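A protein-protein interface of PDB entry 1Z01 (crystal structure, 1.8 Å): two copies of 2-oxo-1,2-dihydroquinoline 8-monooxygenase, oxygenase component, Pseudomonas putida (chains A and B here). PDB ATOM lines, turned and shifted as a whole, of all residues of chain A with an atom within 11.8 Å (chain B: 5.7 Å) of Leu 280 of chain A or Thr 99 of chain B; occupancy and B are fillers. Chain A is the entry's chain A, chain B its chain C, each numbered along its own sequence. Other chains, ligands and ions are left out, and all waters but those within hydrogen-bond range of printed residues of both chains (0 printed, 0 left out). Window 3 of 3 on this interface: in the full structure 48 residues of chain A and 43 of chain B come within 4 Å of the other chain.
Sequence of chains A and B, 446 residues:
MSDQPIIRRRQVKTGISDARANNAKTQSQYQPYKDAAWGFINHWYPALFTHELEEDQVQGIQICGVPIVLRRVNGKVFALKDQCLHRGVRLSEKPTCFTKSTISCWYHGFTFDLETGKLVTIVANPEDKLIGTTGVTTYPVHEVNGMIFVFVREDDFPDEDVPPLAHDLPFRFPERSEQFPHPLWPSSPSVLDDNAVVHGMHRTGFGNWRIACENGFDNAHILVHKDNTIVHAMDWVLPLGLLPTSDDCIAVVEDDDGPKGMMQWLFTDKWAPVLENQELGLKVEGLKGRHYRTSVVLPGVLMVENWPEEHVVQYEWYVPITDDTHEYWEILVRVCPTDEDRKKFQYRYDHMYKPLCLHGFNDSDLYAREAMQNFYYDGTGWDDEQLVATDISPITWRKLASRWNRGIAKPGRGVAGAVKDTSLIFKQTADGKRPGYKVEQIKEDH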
ATOM      1  N   LEU A 223      17.544 -21.102   9.157  1.00  0.00           N
ATOM      2  CA  LEU A 223      17.864 -21.848  10.371  1.00  0.00           C
ATOM      3  C   LEU A 223      16.752 -21.766  11.416  1.00  0.00           C
ATOM      4  O   LEU A 223      16.574 -22.677  12.221  1.00  0.00           O
ATOM      5  CB  LEU A 223      19.167 -21.303  10.961  1.00  0.00           C
ATOM      6  CG  LEU A 223      20.325 -22.287  11.138  1.00  0.00           C
ATOM      7  CD1 LEU A 223      21.663 -21.582  10.888  1.00  0.00           C
ATOM      8  CD2 LEU A 223      20.258 -22.885  12.539  1.00  0.00           C
ATOM      9  N   LYS A 226      14.344 -24.710  11.088  1.00  0.00           N
ATOM     10  CA  LYS A 226      14.908 -26.058  11.127  1.00  0.00           C
ATOM     11  C   LYS A 226      14.075 -27.084  11.891  1.00  0.00           C
ATOM     12  O   LYS A 226      14.019 -28.246  11.500  1.00  0.00           O
ATOM     13  CB  LYS A 226      16.320 -26.029  11.719  1.00  0.00           C
ATOM     14  CG  LYS A 226      16.360 -25.623  13.183  1.00  0.00           C
ATOM     15  CD  LYS A 226      17.763 -25.723  13.775  1.00  0.00           C
ATOM     16  CE  LYS A 226      18.283 -27.154  13.830  1.00  0.00           C
ATOM     17  NZ  LYS A 226      18.511 -27.753  12.486  1.00  0.00           N
ATOM     18  N   LEU A 240      21.272 -25.370   4.832  1.00  0.00           N
ATOM     19  CA  LEU A 240      21.683 -24.467   5.906  1.00  0.00           C
ATOM     20  C   LEU A 240      21.171 -23.053   5.600  1.00  0.00           C
ATOM     21  O   LEU A 240      20.718 -22.335   6.494  1.00  0.00           O
ATOM     22  CB  LEU A 240      23.209 -24.469   6.041  1.00  0.00           C
ATOM     23  CG  LEU A 240      23.847 -25.845   6.293  1.00  0.00           C
ATOM     24  CD1 LEU A 240      25.349 -25.696   6.417  1.00  0.00           C
ATOM     25  CD2 LEU A 240      23.275 -26.466   7.556  1.00  0.00           C
ATOM     26  N   VAL A 274      23.348 -23.851   0.699  1.00  0.00           N
ATOM     27  CA  VAL A 274      24.523 -24.289   1.450  1.00  0.00           C
ATOM     28  C   VAL A 274      24.230 -25.635   2.093  1.00  0.00           C
ATOM     29  O   VAL A 274      23.186 -25.820   2.722  1.00  0.00           O
ATOM     30  CB  VAL A 274      24.900 -23.301   2.571  1.00  0.00           C
ATOM     31  CG1 VAL A 274      26.126 -23.799   3.319  1.00  0.00           C
ATOM     32  CG2 VAL A 274      25.165 -21.942   1.990  1.00  0.00           C
ATOM     33  N   LEU A 275      25.161 -26.571   1.941  1.00  0.00           N
ATOM     34  CA  LEU A 275      24.989 -27.904   2.492  1.00  0.00           C
ATOM     35  C   LEU A 275      25.923 -28.226   3.646  1.00  0.00           C
ATOM     36  O   LEU A 275      25.599 -29.059   4.488  1.00  0.00           O
ATOM     37  CB  LEU A 275      25.172 -28.961   1.397  1.00  0.00           C
ATOM     38  CG  LEU A 275      24.082 -29.076   0.322  1.00  0.00           C
ATOM     39  CD1 LEU A 275      24.021 -27.799  -0.493  1.00  0.00           C
ATOM     40  CD2 LEU A 275      24.375 -30.266  -0.582  1.00  0.00           C
ATOM     41  N   GLU A 276      27.074 -27.569   3.703  1.00  0.00           N
ATOM     42  CA  GLU A 276      28.010 -27.884   4.771  1.00  0.00           C
ATOM     43  C   GLU A 276      28.788 -26.744   5.417  1.00  0.00           C
ATOM     44  O   GLU A 276      28.877 -25.634   4.883  1.00  0.00           O
ATOM     45  CB  GLU A 276      28.990 -28.940   4.267  1.00  0.00           C
ATOM     46  CG  GLU A 276      29.653 -28.571   2.963  1.00  0.00           C
ATOM     47  CD  GLU A 276      30.542 -29.672   2.438  1.00  0.00           C
ATOM     48  OE1 GLU A 276      30.023 -30.665   1.898  1.00  0.00           O
ATOM     49  OE2 GLU A 276      31.769 -29.553   2.570  1.00  0.00           O
ATOM     50  N   ASN A 277      29.341 -27.059   6.587  1.00  0.00           N
ATOM     51  CA  ASN A 277      30.148 -26.146   7.380  1.00  0.00           C
ATOM     52  C   ASN A 277      31.250 -27.009   7.990  1.00  0.00           C
ATOM     53  O   ASN A 277      31.005 -27.770   8.929  1.00  0.00           O
ATOM     54  CB  ASN A 277      29.322 -25.512   8.499  1.00  0.00           C
ATOM     55  CG  ASN A 277      30.061 -24.386   9.186  1.00  0.00           C
ATOM     56  OD1 ASN A 277      29.990 -23.234   8.762  1.00  0.00           O
ATOM     57  ND2 ASN A 277      30.799 -24.717  10.237  1.00  0.00           N
ATOM     58  N   GLN A 278      32.458 -26.892   7.455  1.00  0.00           N
ATOM     59  CA  GLN A 278      33.568 -27.693   7.934  1.00  0.00           C
ATOM     60  C   GLN A 278      34.017 -27.339   9.342  1.00  0.00           C
ATOM     61  O   GLN A 278      34.460 -28.206  10.086  1.00  0.00           O
ATOM     62  CB  GLN A 278      34.735 -27.586   6.957  1.00  0.00           C
ATOM     63  CG  GLN A 278      34.321 -27.834   5.513  1.00  0.00           C
ATOM     64  CD  GLN A 278      35.466 -28.280   4.647  1.00  0.00           C
ATOM     65  OE1 GLN A 278      36.433 -27.549   4.454  1.00  0.00           O
ATOM     66  NE2 GLN A 278      35.372 -29.499   4.129  1.00  0.00           N
ATOM     67  N   GLU A 279      33.908 -26.072   9.719  1.00  0.00           N
ATOM     68  CA  GLU A 279      34.322 -25.679  11.058  1.00  0.00           C
ATOM     69  C   GLU A 279      33.545 -26.475  12.114  1.00  0.00           C
ATOM     70  O   GLU A 279      34.140 -27.117  12.968  1.00  0.00           O
ATOM     71  CB  GLU A 279      34.115 -24.175  11.249  1.00  0.00           C
ATOM     72  CG  GLU A 279      34.654 -23.605  12.559  1.00  0.00           C
ATOM     73  CD  GLU A 279      36.150 -23.807  12.740  1.00  0.00           C
ATOM     74  OE1 GLU A 279      36.917 -23.494  11.808  1.00  0.00           O
ATOM     75  OE2 GLU A 279      36.558 -24.270  13.824  1.00  0.00           O
ATOM     76  N   LEU A 280      32.219 -26.445  12.042  1.00  0.00           N
ATOM     77  CA  LEU A 280      31.372 -27.168  12.984  1.00  0.00           C
ATOM     78  C   LEU A 280      31.199 -28.629  12.591  1.00  0.00           C
ATOM     79  O   LEU A 280      30.704 -29.442  13.372  1.00  0.00           O
ATOM     80  CB  LEU A 280      30.008 -26.502  13.047  1.00  0.00           C
ATOM     81  CG  LEU A 280      29.825 -25.259  13.914  1.00  0.00           C
ATOM     82  CD1 LEU A 280      31.060 -24.348  13.868  1.00  0.00           C
ATOM     83  CD2 LEU A 280      28.564 -24.542  13.416  1.00  0.00           C
ATOM     84  N   GLY A 281      31.600 -28.960  11.371  1.00  0.00           N
ATOM     85  CA  GLY A 281      31.467 -30.333  10.910  1.00  0.00           C
ATOM     86  C   GLY A 281      30.045 -30.693  10.495  1.00  0.00           C
ATOM     87  O   GLY A 281      29.617 -31.837  10.654  1.00  0.00           O
ATOM     88  N   LEU A 282      29.310 -29.710   9.977  1.00  0.00           N
ATOM     89  CA  LEU A 282      27.925 -29.895   9.533  1.00  0.00           C
ATOM     90  C   LEU A 282      27.888 -30.095   8.025  1.00  0.00           C
ATOM     91  O   LEU A 282      28.730 -29.518   7.325  1.00  0.00           O
ATOM     92  CB  LEU A 282      27.099 -28.679   9.855  1.00  0.00           C
ATOM     93  CG  LEU A 282      26.762 -28.484  11.311  1.00  0.00           C
ATOM     94  CD1 LEU A 282      26.016 -27.201  11.386  1.00  0.00           C
ATOM     95  CD2 LEU A 282      25.954 -29.645  11.867  1.00  0.00           C
ATOM     96  N   LYS A 283      26.912 -30.880   7.536  1.00  0.00           N
ATOM     97  CA  LYS A 283      26.767 -31.219   6.112  1.00  0.00           C
ATOM     98  C   LYS A 283      25.438 -31.884   5.859  1.00  0.00           C
ATOM     99  O   LYS A 283      25.134 -32.839   6.536  1.00  0.00           O
ATOM    100  CB  LYS A 283      27.866 -32.195   5.722  1.00  0.00           C
ATOM    101  CG  LYS A 283      27.290 -33.620   5.201  1.00  0.00           C
ATOM    102  CD  LYS A 283      27.414 -34.898   6.064  1.00  0.00           C
ATOM    103  CE  LYS A 283      27.770 -34.730   7.491  1.00  0.00           C
ATOM    104  NZ  LYS A 283      28.237 -35.947   8.133  1.00  0.00           N
ATOM    105  N   VAL A 284      24.735 -31.484   4.806  1.00  0.00           N
ATOM    106  CA  VAL A 284      23.396 -31.997   4.549  1.00  0.00           C
ATOM    107  C   VAL A 284      23.520 -32.800   3.296  1.00  0.00           C
ATOM    108  O   VAL A 284      24.173 -32.383   2.370  1.00  0.00           O
ATOM    109  CB  VAL A 284      22.456 -30.784   4.320  1.00  0.00           C
ATOM    110  CG1 VAL A 284      21.176 -31.193   3.532  1.00  0.00           C
ATOM    111  CG2 VAL A 284      22.190 -30.044   5.604  1.00  0.00           C
ATOM    112  N   ARG B  71      27.425 -21.025  29.479  1.00  0.00           N
ATOM    113  CA  ARG B  71      27.202 -22.405  29.085  1.00  0.00           C
ATOM    114  C   ARG B  71      28.193 -23.294  29.817  1.00  0.00           C
ATOM    115  O   ARG B  71      29.347 -22.923  29.999  1.00  0.00           O
ATOM    116  CB  ARG B  71      27.395 -22.589  27.574  1.00  0.00           C
ATOM    117  CG  ARG B  71      27.130 -24.017  27.102  1.00  0.00           C
ATOM    118  CD  ARG B  71      27.567 -24.266  25.672  1.00  0.00           C
ATOM    119  NE  ARG B  71      27.272 -25.642  25.268  1.00  0.00           N
ATOM    120  CZ  ARG B  71      27.796 -26.250  24.206  1.00  0.00           C
ATOM    121  NH1 ARG B  71      27.459 -27.502  23.931  1.00  0.00           N
ATOM    122  NH2 ARG B  71      28.666 -25.621  23.425  1.00  0.00           N
ATOM    123  N   CYS B  97      23.910 -24.840  20.078  1.00  0.00           N
ATOM    124  CA  CYS B  97      25.343 -25.136  20.063  1.00  0.00           C
ATOM    125  C   CYS B  97      25.602 -26.401  19.253  1.00  0.00           C
ATOM    126  O   CYS B  97      25.067 -27.462  19.569  1.00  0.00           O
ATOM    127  CB  CYS B  97      25.859 -25.331  21.486  1.00  0.00           C
ATOM    128  SG  CYS B  97      25.521 -23.950  22.616  1.00  0.00           S
ATOM    129  N   PHE B  98      26.421 -26.298  18.210  1.00  0.00           N
ATOM    130  CA  PHE B  98      26.699 -27.461  17.376  1.00  0.00           C
ATOM    131  C   PHE B  98      27.925 -28.250  17.795  1.00  0.00           C
ATOM    132  O   PHE B  98      28.059 -29.420  17.442  1.00  0.00           O
ATOM    133  CB  PHE B  98      26.821 -27.045  15.913  1.00  0.00           C
ATOM    134  CG  PHE B  98      25.588 -26.397  15.373  1.00  0.00           C
ATOM    135  CD1 PHE B  98      25.463 -25.015  15.354  1.00  0.00           C
ATOM    136  CD2 PHE B  98      24.531 -27.171  14.913  1.00  0.00           C
ATOM    137  CE1 PHE B  98      24.301 -24.413  14.884  1.00  0.00           C
ATOM    138  CE2 PHE B  98      23.366 -26.578  14.444  1.00  0.00           C
ATOM    139  CZ  PHE B  98      23.252 -25.197  14.428  1.00  0.00           C
ATOM    140  N   THR B  99      28.825 -27.610  18.537  1.00  0.00           N
ATOM    141  CA  THR B  99      30.033 -28.280  19.006  1.00  0.00           C
ATOM    142  C   THR B  99      30.335 -27.885  20.448  1.00  0.00           C
ATOM    143  O   THR B  99      29.834 -26.879  20.952  1.00  0.00           O
ATOM    144  CB  THR B  99      31.261 -27.938  18.134  1.00  0.00           C
ATOM    145  OG1 THR B  99      31.702 -26.609  18.429  1.00  0.00           O
ATOM    146  CG2 THR B  99      30.911 -28.042  16.649  1.00  0.00           C
ATOM    147  N   LYS B 100      31.168 -28.688  21.099  1.00  0.00           N
ATOM    148  CA  LYS B 100      31.549 -28.477  22.490  1.00  0.00           C
ATOM    149  C   LYS B 100      32.315 -27.187  22.749  1.00  0.00           C
ATOM    150  O   LYS B 100      32.338 -26.690  23.872  1.00  0.00           O
ATOM    151  CB  LYS B 100      32.409 -29.650  22.974  1.00  0.00           C
ATOM    152  CG  LYS B 100      31.665 -30.961  23.169  1.00  0.00           C
ATOM    153  CD  LYS B 100      30.785 -30.927  24.409  1.00  0.00           C
ATOM    154  CE  LYS B 100      30.446 -32.341  24.890  1.00  0.00           C
ATOM    155  NZ  LYS B 100      29.710 -33.158  23.878  1.00  0.00           N
ATOM    156  N   SER B 101      32.947 -26.646  21.718  1.00  0.00           N
ATOM    157  CA  SER B 101      33.736 -25.436  21.886  1.00  0.00           C
ATOM    158  C   SER B 101      33.084 -24.153  21.384  1.00  0.00           C
ATOM    159  O   SER B 101      33.736 -23.119  21.332  1.00  0.00           O
ATOM    160  CB  SER B 101      35.088 -25.607  21.188  1.00  0.00           C
ATOM    161  OG  SER B 101      34.916 -25.688  19.784  1.00  0.00           O
ATOM    162  N   THR B 102      31.809 -24.201  21.018  1.00  0.00           N
ATOM    163  CA  THR B 102      31.174 -22.995  20.511  1.00  0.00           C
ATOM    164  C   THR B 102      29.716 -22.803  20.922  1.00  0.00           C
ATOM    165  O   THR B 102      29.119 -23.629  21.611  1.00  0.00           O
ATOM    166  CB  THR B 102      31.222 -22.956  18.963  1.00  0.00           C
ATOM    167  OG1 THR B 102      30.470 -24.059  18.433  1.00  0.00           O
ATOM    168  CG2 THR B 102      32.656 -23.031  18.460  1.00  0.00           C
ATOM    169  N   ILE B 103      29.171 -21.672  20.491  1.00  0.00           N
ATOM    170  CA  ILE B 103      27.781 -21.326  20.707  1.00  0.00           C
ATOM    171  C   ILE B 103      27.392 -20.530  19.470  1.00  0.00           C
ATOM    172  O   ILE B 103      28.118 -19.625  19.059  1.00  0.00           O
ATOM    173  CB  ILE B 103      27.574 -20.472  21.964  1.00  0.00           C
ATOM    174  CG1 ILE B 103      26.081 -20.169  22.128  1.00  0.00           C
ATOM    175  CG2 ILE B 103      28.382 -19.195  21.874  1.00  0.00           C
ATOM    176  CD1 ILE B 103      25.721 -19.624  23.492  1.00  0.00           C
ATOM    177  N   SER B 104      26.268 -20.884  18.857  1.00  0.00           N
ATOM    178  CA  SER B 104      25.827 -20.196  17.650  1.00  0.00           C
ATOM    179  C   SER B 104      24.575 -19.366  17.868  1.00  0.00           C
ATOM    180  O   SER B 104      23.827 -19.569  18.831  1.00  0.00           O
ATOM    181  CB  SER B 104      25.549 -21.210  16.536  1.00  0.00           C
ATOM    182  OG  SER B 104      26.708 -21.956  16.227  1.00  0.00           O
ATOM    183  N   THR B 111      28.627 -18.003  14.540  1.00  0.00           N
ATOM    184  CA  THR B 111      29.100 -18.927  15.563  1.00  0.00           C
ATOM    185  C   THR B 111      30.359 -18.417  16.251  1.00  0.00           C
ATOM    186  O   THR B 111      31.307 -17.981  15.588  1.00  0.00           O
ATOM    187  CB  THR B 111      29.371 -20.294  14.939  1.00  0.00           C
ATOM    188  OG1 THR B 111      28.166 -20.773  14.329  1.00  0.00           O
ATOM    189  CG2 THR B 111      29.832 -21.287  15.991  1.00  0.00           C
ATOM    190  N   LEU B 114      33.748 -20.382  22.423  1.00  0.00           N
ATOM    191  CA  LEU B 114      33.478 -20.148  23.842  1.00  0.00           C
ATOM    192  C   LEU B 114      34.662 -19.573  24.617  1.00  0.00           C
ATOM    193  O   LEU B 114      34.486 -18.732  25.501  1.00  0.00           O
ATOM    194  CB  LEU B 114      33.032 -21.449  24.518  1.00  0.00           C
ATOM    195  CG  LEU B 114      31.686 -22.060  24.127  1.00  0.00           C
ATOM    196  CD1 LEU B 114      31.538 -23.441  24.752  1.00  0.00           C
ATOM    197  CD2 LEU B 114      30.566 -21.142  24.584  1.00  0.00           C
ATOM    198  N   VAL B 120      34.105 -17.726  14.669  1.00  0.00           N
ATOM    199  CA  VAL B 120      34.801 -18.796  13.969  1.00  0.00           C
ATOM    200  C   VAL B 120      34.180 -19.222  12.655  1.00  0.00           C
ATOM    201  O   VAL B 120      34.837 -19.866  11.841  1.00  0.00           O
ATOM    202  CB  VAL B 120      34.956 -20.030  14.873  1.00  0.00           C
ATOM    203  CG1 VAL B 120      35.812 -19.685  16.068  1.00  0.00           C
ATOM    204  CG2 VAL B 120      33.612 -20.509  15.329  1.00  0.00           C
ATOM    205  N   THR B 121      32.914 -18.879  12.449  1.00  0.00           N
ATOM    206  CA  THR B 121      32.234 -19.215  11.200  1.00  0.00           C
ATOM    207  C   THR B 121      30.776 -18.761  11.210  1.00  0.00           C
ATOM    208  O   THR B 121      30.284 -18.228  12.201  1.00  0.00           O
ATOM    209  CB  THR B 121      32.257 -20.737  10.926  1.00  0.00           C
ATOM    210  OG1 THR B 121      31.744 -20.999   9.613  1.00  0.00           O
ATOM    211  CG2 THR B 121      31.390 -21.468  11.939  1.00  0.00           C
ATOM    212  N   VAL B 123      27.256 -20.569  10.003  1.00  0.00           N
ATOM    213  CA  VAL B 123      26.649 -21.808   9.531  1.00  0.00           C
ATOM    214  C   VAL B 123      26.434 -21.958   8.019  1.00  0.00           C
ATOM    215  O   VAL B 123      26.973 -22.880   7.405  1.00  0.00           O
ATOM    216  CB  VAL B 123      25.313 -22.064  10.258  1.00  0.00           C
ATOM    217  CG1 VAL B 123      24.746 -23.420   9.855  1.00  0.00           C
ATOM    218  CG2 VAL B 123      25.529 -22.005  11.768  1.00  0.00           C
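The side-chain amide oxygen (OD1) of Asn 277 of chain A sits at hydrogen-bond distance from the side-chain hydroxyl (OG1) of Thr 121 of chain B, at 3.0 Å. The side-chain amide oxygen of Asn 277 of chain A sits close to the backbone carbonyl oxygen of Val 123 of chain B, 3.3 Å away.
The backbone NH of Leu 240 of chain A is in hydrogen-bond range of the backbone carbonyl oxygen of Val 274 of chain A (2.9 Å). ND2 of Asn 277 of chain A lies close to N of Glu 279 of chain A, at 3.4 Å. The backbone NH (N) of Leu 280 of chain A lies close to the side-chain amide nitrogen (ND2) of Asn 277 of chain A, 2.9 Å away. The backbone NH (N) of Asn 277 of chain A lies within hydrogen-bond range of the backbone carbonyl oxygen (O) of Leu 282 of chain A, 2.6 Å away. The guanidinium group (NH2) of Arg 71 of chain B sits at hydrogen-bond distance from the backbone carbonyl oxygen (O) of Thr 99 of chain B (3.0 Å). N of Val 120 of chain B is in hydrogen-bond range of O of Thr 111 of chain B.
Among the printed residues, merely in contact across the chains: Leu 223 of chain A with Val 123 of chain B (3.7 Å), Leu 240 of chain A with Val 123 of chain B (3.4 Å), Glu 279 of chain A with Val 120 of chain B (3.8 Å), Glu 279 of chain A with Thr 121 of chain B (3.9 Å), Leu 280 of chain A with Phe 98 of chain B (3.7 Å), Leu 280 of chain A with Thr 99 of chain B (3.6 Å), Leu 280 of chain A with Thr 111 of chain B (3.9 Å), Leu 280 of chain A with Thr 121 of chain B (3.5 Å) and Leu 282 of chain A with Phe 98 of chain B (3.8 Å).
Of the printed residues of chain B, Leu 280 of chain A touches Phe 98, Thr 99, Thr 111 and Thr 121. Thr 99 of chain B touches just one residue of chain A: Leu 280 (3.6 Å). Cys 97 of chain B touches none of the printed residues of chain A. Phe 98 of chain B touches just these residues of chain A: Leu 280 (3.7 Å) and Leu 282 (3.8 Å). No residue of chain A comes within 4 Å of Lys 100 of chain B. Ser 101 of chain B touches none of the printed residues of chain A. No residue of chain A comes within 4 Å of Thr 102 of chain B. Thr 111 of chain B touches just one residue of chain A: Leu 280 (3.9 Å). Printed residues of chain B within 4 Å of Asn 277 of chain A: Thr 121 (3.0 Å) and Val 123 (3.3 Å). Of the printed residues of chain B, Leu 223 of chain A touches Val 123 (3.7 Å). Of the printed residues of chain B, Glu 279 of chain A touches Val 120 (3.8 Å) and Thr 121 (3.9 Å). Of the printed residues of chain B, Leu 282 of chain A touches Phe 98 (3.8 Å). Of the printed residues of chain B, Leu 240 of chain A touches Val 123.
Of the 14 printed residues of chain B, 6 touch a printed residue of chain A. Along chain B the printed residues that touch a printed residue of chain A span positions 98 to 123.
No position is printed for both chains.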
